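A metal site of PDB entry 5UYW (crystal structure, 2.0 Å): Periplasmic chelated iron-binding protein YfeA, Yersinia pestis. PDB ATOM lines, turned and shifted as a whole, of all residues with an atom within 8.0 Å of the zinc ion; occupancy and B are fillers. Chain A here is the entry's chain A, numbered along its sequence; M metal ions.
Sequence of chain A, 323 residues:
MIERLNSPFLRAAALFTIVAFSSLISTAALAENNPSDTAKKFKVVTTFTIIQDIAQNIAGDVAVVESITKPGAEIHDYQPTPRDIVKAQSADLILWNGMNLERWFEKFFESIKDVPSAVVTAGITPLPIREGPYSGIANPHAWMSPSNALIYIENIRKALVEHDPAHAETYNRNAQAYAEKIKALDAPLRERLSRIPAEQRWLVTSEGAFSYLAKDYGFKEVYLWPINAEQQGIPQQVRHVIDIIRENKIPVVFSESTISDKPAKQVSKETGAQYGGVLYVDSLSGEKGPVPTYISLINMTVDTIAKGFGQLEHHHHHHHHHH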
ATOM      1  N   PHE A  48       6.443 -24.060  13.271  1.00  0.00           N
ATOM      2  CA  PHE A  48       7.121 -24.009  11.971  1.00  0.00           C
ATOM      3  C   PHE A  48       7.343 -22.556  11.541  1.00  0.00           C
ATOM      4  O   PHE A  48       6.971 -21.610  12.246  1.00  0.00           O
ATOM      5  CB  PHE A  48       6.389 -24.851  10.904  1.00  0.00           C
ATOM      6  CG  PHE A  48       5.107 -24.249  10.367  1.00  0.00           C
ATOM      7  CD1 PHE A  48       4.008 -24.096  11.170  1.00  0.00           C
ATOM      8  CD2 PHE A  48       4.999 -23.931   9.020  1.00  0.00           C
ATOM      9  CE1 PHE A  48       2.841 -23.582  10.669  1.00  0.00           C
ATOM     10  CE2 PHE A  48       3.824 -23.416   8.508  1.00  0.00           C
ATOM     11  CZ  PHE A  48       2.731 -23.243   9.333  1.00  0.00           C
ATOM     12  N   GLU A  74      10.303 -30.955   6.441  1.00  0.00           N
ATOM     13  CA  GLU A  74       8.914 -31.379   6.267  1.00  0.00           C
ATOM     14  C   GLU A  74       8.184 -31.234   7.598  1.00  0.00           C
ATOM     15  O   GLU A  74       8.645 -31.746   8.611  1.00  0.00           O
ATOM     16  CB  GLU A  74       8.885 -32.832   5.782  1.00  0.00           C
ATOM     17  CG  GLU A  74       7.680 -33.213   4.953  1.00  0.00           C
ATOM     18  CD  GLU A  74       6.411 -33.287   5.772  1.00  0.00           C
ATOM     19  OE1 GLU A  74       6.352 -34.146   6.681  1.00  0.00           O
ATOM     20  OE2 GLU A  74       5.490 -32.484   5.506  1.00  0.00           O
ATOM     21  N   ILE A  75       7.047 -30.531   7.598  1.00  0.00           N
ATOM     22  CA  ILE A  75       6.422 -30.152   8.863  1.00  0.00           C
ATOM     23  C   ILE A  75       5.278 -31.071   9.294  1.00  0.00           C
ATOM     24  O   ILE A  75       4.957 -31.113  10.491  1.00  0.00           O
ATOM     25  CB  ILE A  75       5.898 -28.700   8.811  1.00  0.00           C
ATOM     26  CG1 ILE A  75       4.767 -28.579   7.761  1.00  0.00           C
ATOM     27  CG2 ILE A  75       7.028 -27.734   8.501  1.00  0.00           C
ATOM     28  CD1 ILE A  75       4.195 -27.175   7.644  1.00  0.00           C
ATOM     29  N   HIS A  76       4.608 -31.760   8.351  1.00  0.00           N
ATOM     30  CA  HIS A  76       3.413 -32.530   8.725  1.00  0.00           C
ATOM     31  C   HIS A  76       3.774 -33.718   9.609  1.00  0.00           C
ATOM     32  O   HIS A  76       3.097 -33.996  10.588  1.00  0.00           O
ATOM     33  CB  HIS A  76       2.688 -33.045   7.485  1.00  0.00           C
ATOM     34  CG  HIS A  76       2.110 -31.975   6.605  1.00  0.00           C
ATOM     35  ND1 HIS A  76       0.762 -31.703   6.549  1.00  0.00           N
ATOM     36  CD2 HIS A  76       2.698 -31.158   5.690  1.00  0.00           C
ATOM     37  CE1 HIS A  76       0.543 -30.749   5.666  1.00  0.00           C
ATOM     38  NE2 HIS A  76       1.706 -30.399   5.130  1.00  0.00           N
ATOM     39  N   LEU A 101      -2.384 -29.803  11.317  1.00  0.00           N
ATOM     40  CA  LEU A 101      -1.212 -29.695  10.445  1.00  0.00           C
ATOM     41  C   LEU A 101      -0.045 -30.488  11.025  1.00  0.00           C
ATOM     42  O   LEU A 101       0.521 -31.371  10.368  1.00  0.00           O
ATOM     43  CB  LEU A 101      -0.811 -28.221  10.288  1.00  0.00           C
ATOM     44  CG  LEU A 101       0.553 -28.023   9.620  1.00  0.00           C
ATOM     45  CD1 LEU A 101       0.430 -28.396   8.129  1.00  0.00           C
ATOM     46  CD2 LEU A 101       1.060 -26.574   9.772  1.00  0.00           C
ATOM     47  N   ASN A 139      -8.213 -29.089   5.431  1.00  0.00           N
ATOM     48  CA  ASN A 139      -6.957 -28.729   4.743  1.00  0.00           C
ATOM     49  C   ASN A 139      -6.235 -27.705   5.611  1.00  0.00           C
ATOM     50  O   ASN A 139      -6.780 -26.612   5.840  1.00  0.00           O
ATOM     51  CB  ASN A 139      -7.232 -28.159   3.362  1.00  0.00           C
ATOM     52  CG  ASN A 139      -5.972 -27.889   2.563  1.00  0.00           C
ATOM     53  OD1 ASN A 139      -4.948 -27.433   3.101  1.00  0.00           O
ATOM     54  ND2 ASN A 139      -6.023 -28.191   1.251  1.00  0.00           N
ATOM     55  N   PRO A 140      -5.046 -27.997   6.129  1.00  0.00           N
ATOM     56  CA  PRO A 140      -4.452 -27.129   7.169  1.00  0.00           C
ATOM     57  C   PRO A 140      -3.725 -25.893   6.633  1.00  0.00           C
ATOM     58  O   PRO A 140      -3.353 -25.026   7.444  1.00  0.00           O
ATOM     59  CB  PRO A 140      -3.467 -28.070   7.871  1.00  0.00           C
ATOM     60  CG  PRO A 140      -3.032 -29.023   6.763  1.00  0.00           C
ATOM     61  CD  PRO A 140      -4.223 -29.194   5.856  1.00  0.00           C
ATOM     62  N   HIS A 141      -3.515 -25.781   5.318  1.00  0.00           N
ATOM     63  CA  HIS A 141      -2.688 -24.718   4.739  1.00  0.00           C
ATOM     64  C   HIS A 141      -3.438 -23.391   4.605  1.00  0.00           C
ATOM     65  O   HIS A 141      -3.415 -22.755   3.542  1.00  0.00           O
ATOM     66  CB  HIS A 141      -2.153 -25.159   3.360  1.00  0.00           C
ATOM     67  CG  HIS A 141      -1.423 -26.472   3.374  1.00  0.00           C
ATOM     68  ND1 HIS A 141      -2.022 -27.678   3.046  1.00  0.00           N
ATOM     69  CD2 HIS A 141      -0.128 -26.770   3.648  1.00  0.00           C
ATOM     70  CE1 HIS A 141      -1.142 -28.654   3.132  1.00  0.00           C
ATOM     71  NE2 HIS A 141       0.025 -28.138   3.481  1.00  0.00           N
ATOM     72  N   TRP A 143      -2.873 -20.453   5.699  1.00  0.00           N
ATOM     73  CA  TRP A 143      -2.086 -19.235   5.570  1.00  0.00           C
ATOM     74  C   TRP A 143      -1.828 -18.844   4.119  1.00  0.00           C
ATOM     75  O   TRP A 143      -1.348 -17.737   3.876  1.00  0.00           O
ATOM     76  CB  TRP A 143      -0.737 -19.390   6.300  1.00  0.00           C
ATOM     77  CG  TRP A 143       0.120 -20.469   5.727  1.00  0.00           C
ATOM     78  CD1 TRP A 143       1.043 -20.330   4.723  1.00  0.00           C
ATOM     79  CD2 TRP A 143       0.146 -21.855   6.112  1.00  0.00           C
ATOM     80  NE1 TRP A 143       1.634 -21.550   4.471  1.00  0.00           N
ATOM     81  CE2 TRP A 143       1.126 -22.492   5.317  1.00  0.00           C
ATOM     82  CE3 TRP A 143      -0.537 -22.612   7.085  1.00  0.00           C
ATOM     83  CZ2 TRP A 143       1.388 -23.854   5.409  1.00  0.00           C
ATOM     84  CZ3 TRP A 143      -0.240 -23.963   7.206  1.00  0.00           C
ATOM     85  CH2 TRP A 143       0.714 -24.573   6.362  1.00  0.00           C
ATOM     86  N   GLU A 207       1.762 -31.610  -3.614  1.00  0.00           N
ATOM     87  CA  GLU A 207       0.806 -31.578  -2.508  1.00  0.00           C
ATOM     88  C   GLU A 207      -0.350 -30.644  -2.857  1.00  0.00           C
ATOM     89  O   GLU A 207      -0.136 -29.569  -3.438  1.00  0.00           O
ATOM     90  CB  GLU A 207       1.467 -31.113  -1.197  1.00  0.00           C
ATOM     91  CG  GLU A 207       0.518 -31.264   0.017  1.00  0.00           C
ATOM     92  CD  GLU A 207       1.087 -30.725   1.333  1.00  0.00           C
ATOM     93  OE1 GLU A 207       1.973 -29.833   1.344  1.00  0.00           O
ATOM     94  OE2 GLU A 207       0.624 -31.210   2.379  1.00  0.00           O
ATOM     95  N   GLY A 208      -1.573 -31.048  -2.531  1.00  0.00           N
ATOM     96  CA  GLY A 208      -2.697 -30.142  -2.650  1.00  0.00           C
ATOM     97  C   GLY A 208      -2.728 -29.096  -1.541  1.00  0.00           C
ATOM     98  O   GLY A 208      -3.724 -28.940  -0.830  1.00  0.00           O
ATOM     99  N   ALA A 209      -1.634 -28.340  -1.422  1.00  0.00           N
ATOM    100  CA  ALA A 209      -1.461 -27.372  -0.350  1.00  0.00           C
ATOM    101  C   ALA A 209      -1.962 -25.979  -0.698  1.00  0.00           C
ATOM    102  O   ALA A 209      -1.809 -25.054   0.115  1.00  0.00           O
ATOM    103  CB  ALA A 209       0.010 -27.295   0.033  1.00  0.00           C
ATOM    104  N   PHE A 210      -2.537 -25.775  -1.888  1.00  0.00           N
ATOM    105  CA  PHE A 210      -2.791 -24.422  -2.349  1.00  0.00           C
ATOM    106  C   PHE A 210      -4.286 -24.115  -2.459  1.00  0.00           C
ATOM    107  O   PHE A 210      -4.642 -23.104  -3.057  1.00  0.00           O
ATOM    108  CB  PHE A 210      -2.081 -24.188  -3.689  1.00  0.00           C
ATOM    109  CG  PHE A 210      -0.609 -24.320  -3.593  1.00  0.00           C
ATOM    110  CD1 PHE A 210       0.177 -23.214  -3.266  1.00  0.00           C
ATOM    111  CD2 PHE A 210       0.002 -25.558  -3.733  1.00  0.00           C
ATOM    112  CE1 PHE A 210       1.551 -23.336  -3.131  1.00  0.00           C
ATOM    113  CE2 PHE A 210       1.383 -25.691  -3.603  1.00  0.00           C
ATOM    114  CZ  PHE A 210       2.160 -24.571  -3.295  1.00  0.00           C
ATOM    115  N   TRP A 225      -0.918 -35.551  -4.594  1.00  0.00           N
ATOM    116  CA  TRP A 225      -1.452 -36.129  -3.375  1.00  0.00           C
ATOM    117  C   TRP A 225      -2.095 -35.028  -2.551  1.00  0.00           C
ATOM    118  O   TRP A 225      -1.669 -33.875  -2.604  1.00  0.00           O
ATOM    119  CB  TRP A 225      -0.372 -36.874  -2.549  1.00  0.00           C
ATOM    120  CG  TRP A 225       0.854 -36.059  -2.166  1.00  0.00           C
ATOM    121  CD1 TRP A 225       1.048 -35.357  -1.008  1.00  0.00           C
ATOM    122  CD2 TRP A 225       2.070 -35.916  -2.920  1.00  0.00           C
ATOM    123  NE1 TRP A 225       2.288 -34.766  -1.003  1.00  0.00           N
ATOM    124  CE2 TRP A 225       2.942 -35.103  -2.165  1.00  0.00           C
ATOM    125  CE3 TRP A 225       2.508 -36.401  -4.164  1.00  0.00           C
ATOM    126  CZ2 TRP A 225       4.215 -34.750  -2.612  1.00  0.00           C
ATOM    127  CZ3 TRP A 225       3.774 -36.054  -4.607  1.00  0.00           C
ATOM    128  CH2 TRP A 225       4.617 -35.235  -3.833  1.00  0.00           C
ATOM    129  N   PRO A 226      -3.155 -35.342  -1.817  1.00  0.00           N
ATOM    130  CA  PRO A 226      -3.947 -34.262  -1.210  1.00  0.00           C
ATOM    131  C   PRO A 226      -3.284 -33.619  -0.005  1.00  0.00           C
ATOM    132  O   PRO A 226      -3.497 -32.423   0.230  1.00  0.00           O
ATOM    133  CB  PRO A 226      -5.270 -34.960  -0.841  1.00  0.00           C
ATOM    134  CG  PRO A 226      -4.969 -36.418  -0.890  1.00  0.00           C
ATOM    135  CD  PRO A 226      -3.887 -36.619  -1.871  1.00  0.00           C
ATOM    136  N   ILE A 227      -2.486 -34.357   0.758  1.00  0.00           N
ATOM    137  CA  ILE A 227      -1.760 -33.801   1.908  1.00  0.00           C
ATOM    138  C   ILE A 227      -0.540 -34.694   2.168  1.00  0.00           C
ATOM    139  O   ILE A 227      -0.594 -35.913   1.977  1.00  0.00           O
ATOM    140  CB  ILE A 227      -2.689 -33.696   3.145  1.00  0.00           C
ATOM    141  CG1 ILE A 227      -1.987 -33.029   4.327  1.00  0.00           C
ATOM    142  CG2 ILE A 227      -3.261 -35.063   3.537  1.00  0.00           C
ATOM    143  CD1 ILE A 227      -2.950 -32.603   5.449  1.00  0.00           C
ATOM    144  N   ASN A 228       0.563 -34.079   2.566  1.00  0.00           N
ATOM    145  CA  ASN A 228       1.780 -34.846   2.839  1.00  0.00           C
ATOM    146  C   ASN A 228       1.504 -35.911   3.889  1.00  0.00           C
ATOM    147  O   ASN A 228       0.865 -35.643   4.918  1.00  0.00           O
ATOM    148  CB  ASN A 228       2.917 -33.940   3.320  1.00  0.00           C
ATOM    149  CG  ASN A 228       3.447 -33.025   2.239  1.00  0.00           C
ATOM    150  OD1 ASN A 228       3.064 -33.129   1.079  1.00  0.00           O
ATOM    151  ND2 ASN A 228       4.352 -32.115   2.626  1.00  0.00           N
ATOM    152  N   ALA A 229       2.009 -37.121   3.642  1.00  0.00           N
ATOM    153  CA  ALA A 229       1.869 -38.265   4.531  1.00  0.00           C
ATOM    154  C   ALA A 229       2.613 -39.453   3.913  1.00  0.00           C
ATOM    155  O   ALA A 229       3.063 -39.401   2.769  1.00  0.00           O
ATOM    156  CB  ALA A 229       0.397 -38.636   4.759  1.00  0.00           C
ATOM    157  N   GLU A 256       6.949 -28.438  -4.657  1.00  0.00           N
ATOM    158  CA  GLU A 256       7.048 -27.562  -3.502  1.00  0.00           C
ATOM    159  C   GLU A 256       8.343 -27.817  -2.753  1.00  0.00           C
ATOM    160  O   GLU A 256       8.960 -28.876  -2.875  1.00  0.00           O
ATOM    161  CB  GLU A 256       5.850 -27.740  -2.559  1.00  0.00           C
ATOM    162  CG  GLU A 256       4.520 -27.452  -3.224  1.00  0.00           C
ATOM    163  CD  GLU A 256       3.920 -28.695  -3.816  1.00  0.00           C
ATOM    164  OE1 GLU A 256       3.725 -29.671  -3.039  1.00  0.00           O
ATOM    165  OE2 GLU A 256       3.647 -28.704  -5.048  1.00  0.00           O
ATOM    166  N   THR A 258       9.454 -28.474   0.257  1.00  0.00           N
ATOM    167  CA  THR A 258       9.843 -29.443   1.274  1.00  0.00           C
ATOM    168  C   THR A 258       9.693 -30.882   0.825  1.00  0.00           C
ATOM    169  O   THR A 258       9.955 -31.787   1.625  1.00  0.00           O
ATOM    170  CB  THR A 258       9.073 -29.253   2.592  1.00  0.00           C
ATOM    171  OG1 THR A 258       7.696 -29.644   2.446  1.00  0.00           O
ATOM    172  CG2 THR A 258       9.160 -27.808   3.082  1.00  0.00           C
ATOM    173  N   ILE A 259       9.270 -31.120  -0.412  1.00  0.00           N
ATOM    174  CA  ILE A 259       8.981 -32.454  -0.907  1.00  0.00           C
ATOM    175  C   ILE A 259       9.777 -32.685  -2.202  1.00  0.00           C
ATOM    176  O   ILE A 259      10.347 -31.762  -2.778  1.00  0.00           O
ATOM    177  CB  ILE A 259       7.460 -32.690  -1.125  1.00  0.00           C
ATOM    178  CG1 ILE A 259       6.821 -31.507  -1.839  1.00  0.00           C
ATOM    179  CG2 ILE A 259       6.750 -32.929   0.206  1.00  0.00           C
ATOM    180  CD1 ILE A 259       6.776 -31.647  -3.362  1.00  0.00           C
ATOM    181  N   VAL A 281       5.201 -23.232   0.282  1.00  0.00           N
ATOM    182  CA  VAL A 281       3.987 -23.219   1.089  1.00  0.00           C
ATOM    183  C   VAL A 281       4.300 -23.635   2.525  1.00  0.00           C
ATOM    184  O   VAL A 281       3.932 -22.943   3.479  1.00  0.00           O
ATOM    185  CB  VAL A 281       2.898 -24.098   0.435  1.00  0.00           C
ATOM    186  CG1 VAL A 281       3.422 -25.480   0.088  1.00  0.00           C
ATOM    187  CG2 VAL A 281       1.651 -24.226   1.329  1.00  0.00           C
ATOM    188  N   ASP A 282       4.998 -24.756   2.709  1.00  0.00           N
ATOM    189  CA  ASP A 282       5.184 -25.311   4.047  1.00  0.00           C
ATOM    190  C   ASP A 282       6.413 -24.778   4.762  1.00  0.00           C
ATOM    191  O   ASP A 282       6.575 -25.048   5.960  1.00  0.00           O
ATOM    192  CB  ASP A 282       5.262 -26.828   3.993  1.00  0.00           C
ATOM    193  CG  ASP A 282       3.910 -27.459   3.738  1.00  0.00           C
ATOM    194  OD1 ASP A 282       2.900 -26.731   3.759  1.00  0.00           O
ATOM    195  OD2 ASP A 282       3.864 -28.688   3.541  1.00  0.00           O
ATOM    196  N   SER A 283       7.264 -24.012   4.104  1.00  0.00           N
ATOM    197  CA  SER A 283       8.434 -23.526   4.820  1.00  0.00           C
ATOM    198  C   SER A 283       8.934 -22.264   4.154  1.00  0.00           C
ATOM    199  O   SER A 283       8.830 -22.103   2.935  1.00  0.00           O
ATOM    200  CB  SER A 283       9.554 -24.577   4.880  1.00  0.00           C
ATOM    201  OG  SER A 283      10.713 -24.020   5.490  1.00  0.00           O
HETATM  202 ZN    ZN M   1       1.845 -29.201   3.419  1.00  0.00          ZN
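Merely in contact with the zinc ion: Asn 228. Within 4 Å of the zinc ion: His 76, His 141, Glu 207, Asn 228 and Asp 282. The nearest printed residue that does not touch the zinc ion is Ala 209 (4.3 Å).
N of His 76 is in hydrogen-bond range of OE2 of Glu 74, at 3.1 Å. ND1 of His 141 is in hydrogen-bond range of OD1 of Asn 139 (2.9 Å). OE2 of Glu 207 lies close to N of Asn 228. The side-chain carboxylate of Glu 256 is in hydrogen-bond range of the backbone NH of Glu 207 (2.8 Å). The side-chain amide nitrogen (ND2) of Asn 228 lies within hydrogen-bond range of the side-chain carboxylate (OE2) of Glu 74. The side-chain amide oxygen (OD1) of Asn 228 sits at hydrogen-bond distance from the indole nitrogen (NE1) of Trp 225 (2.8 Å).
The zinc ion is bound by the side-chain carboxylate (OD2) of Asp 282, at 2.1 Å. The zinc ion is bound by NE2 of His 76 (2.1 Å). NE2 of His 141 binds the zinc ion. The zinc ion is bound by OE1 of Glu 207. The side-chain carboxylate (OE2) of Glu 207 binds the zinc ion, 2.6 Å away. The zinc ion has five donor atoms within binding distance. Slightly farther from the zinc ion lies the side-chain carboxylate (OD1) of Asp 282 (2.7 Å).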
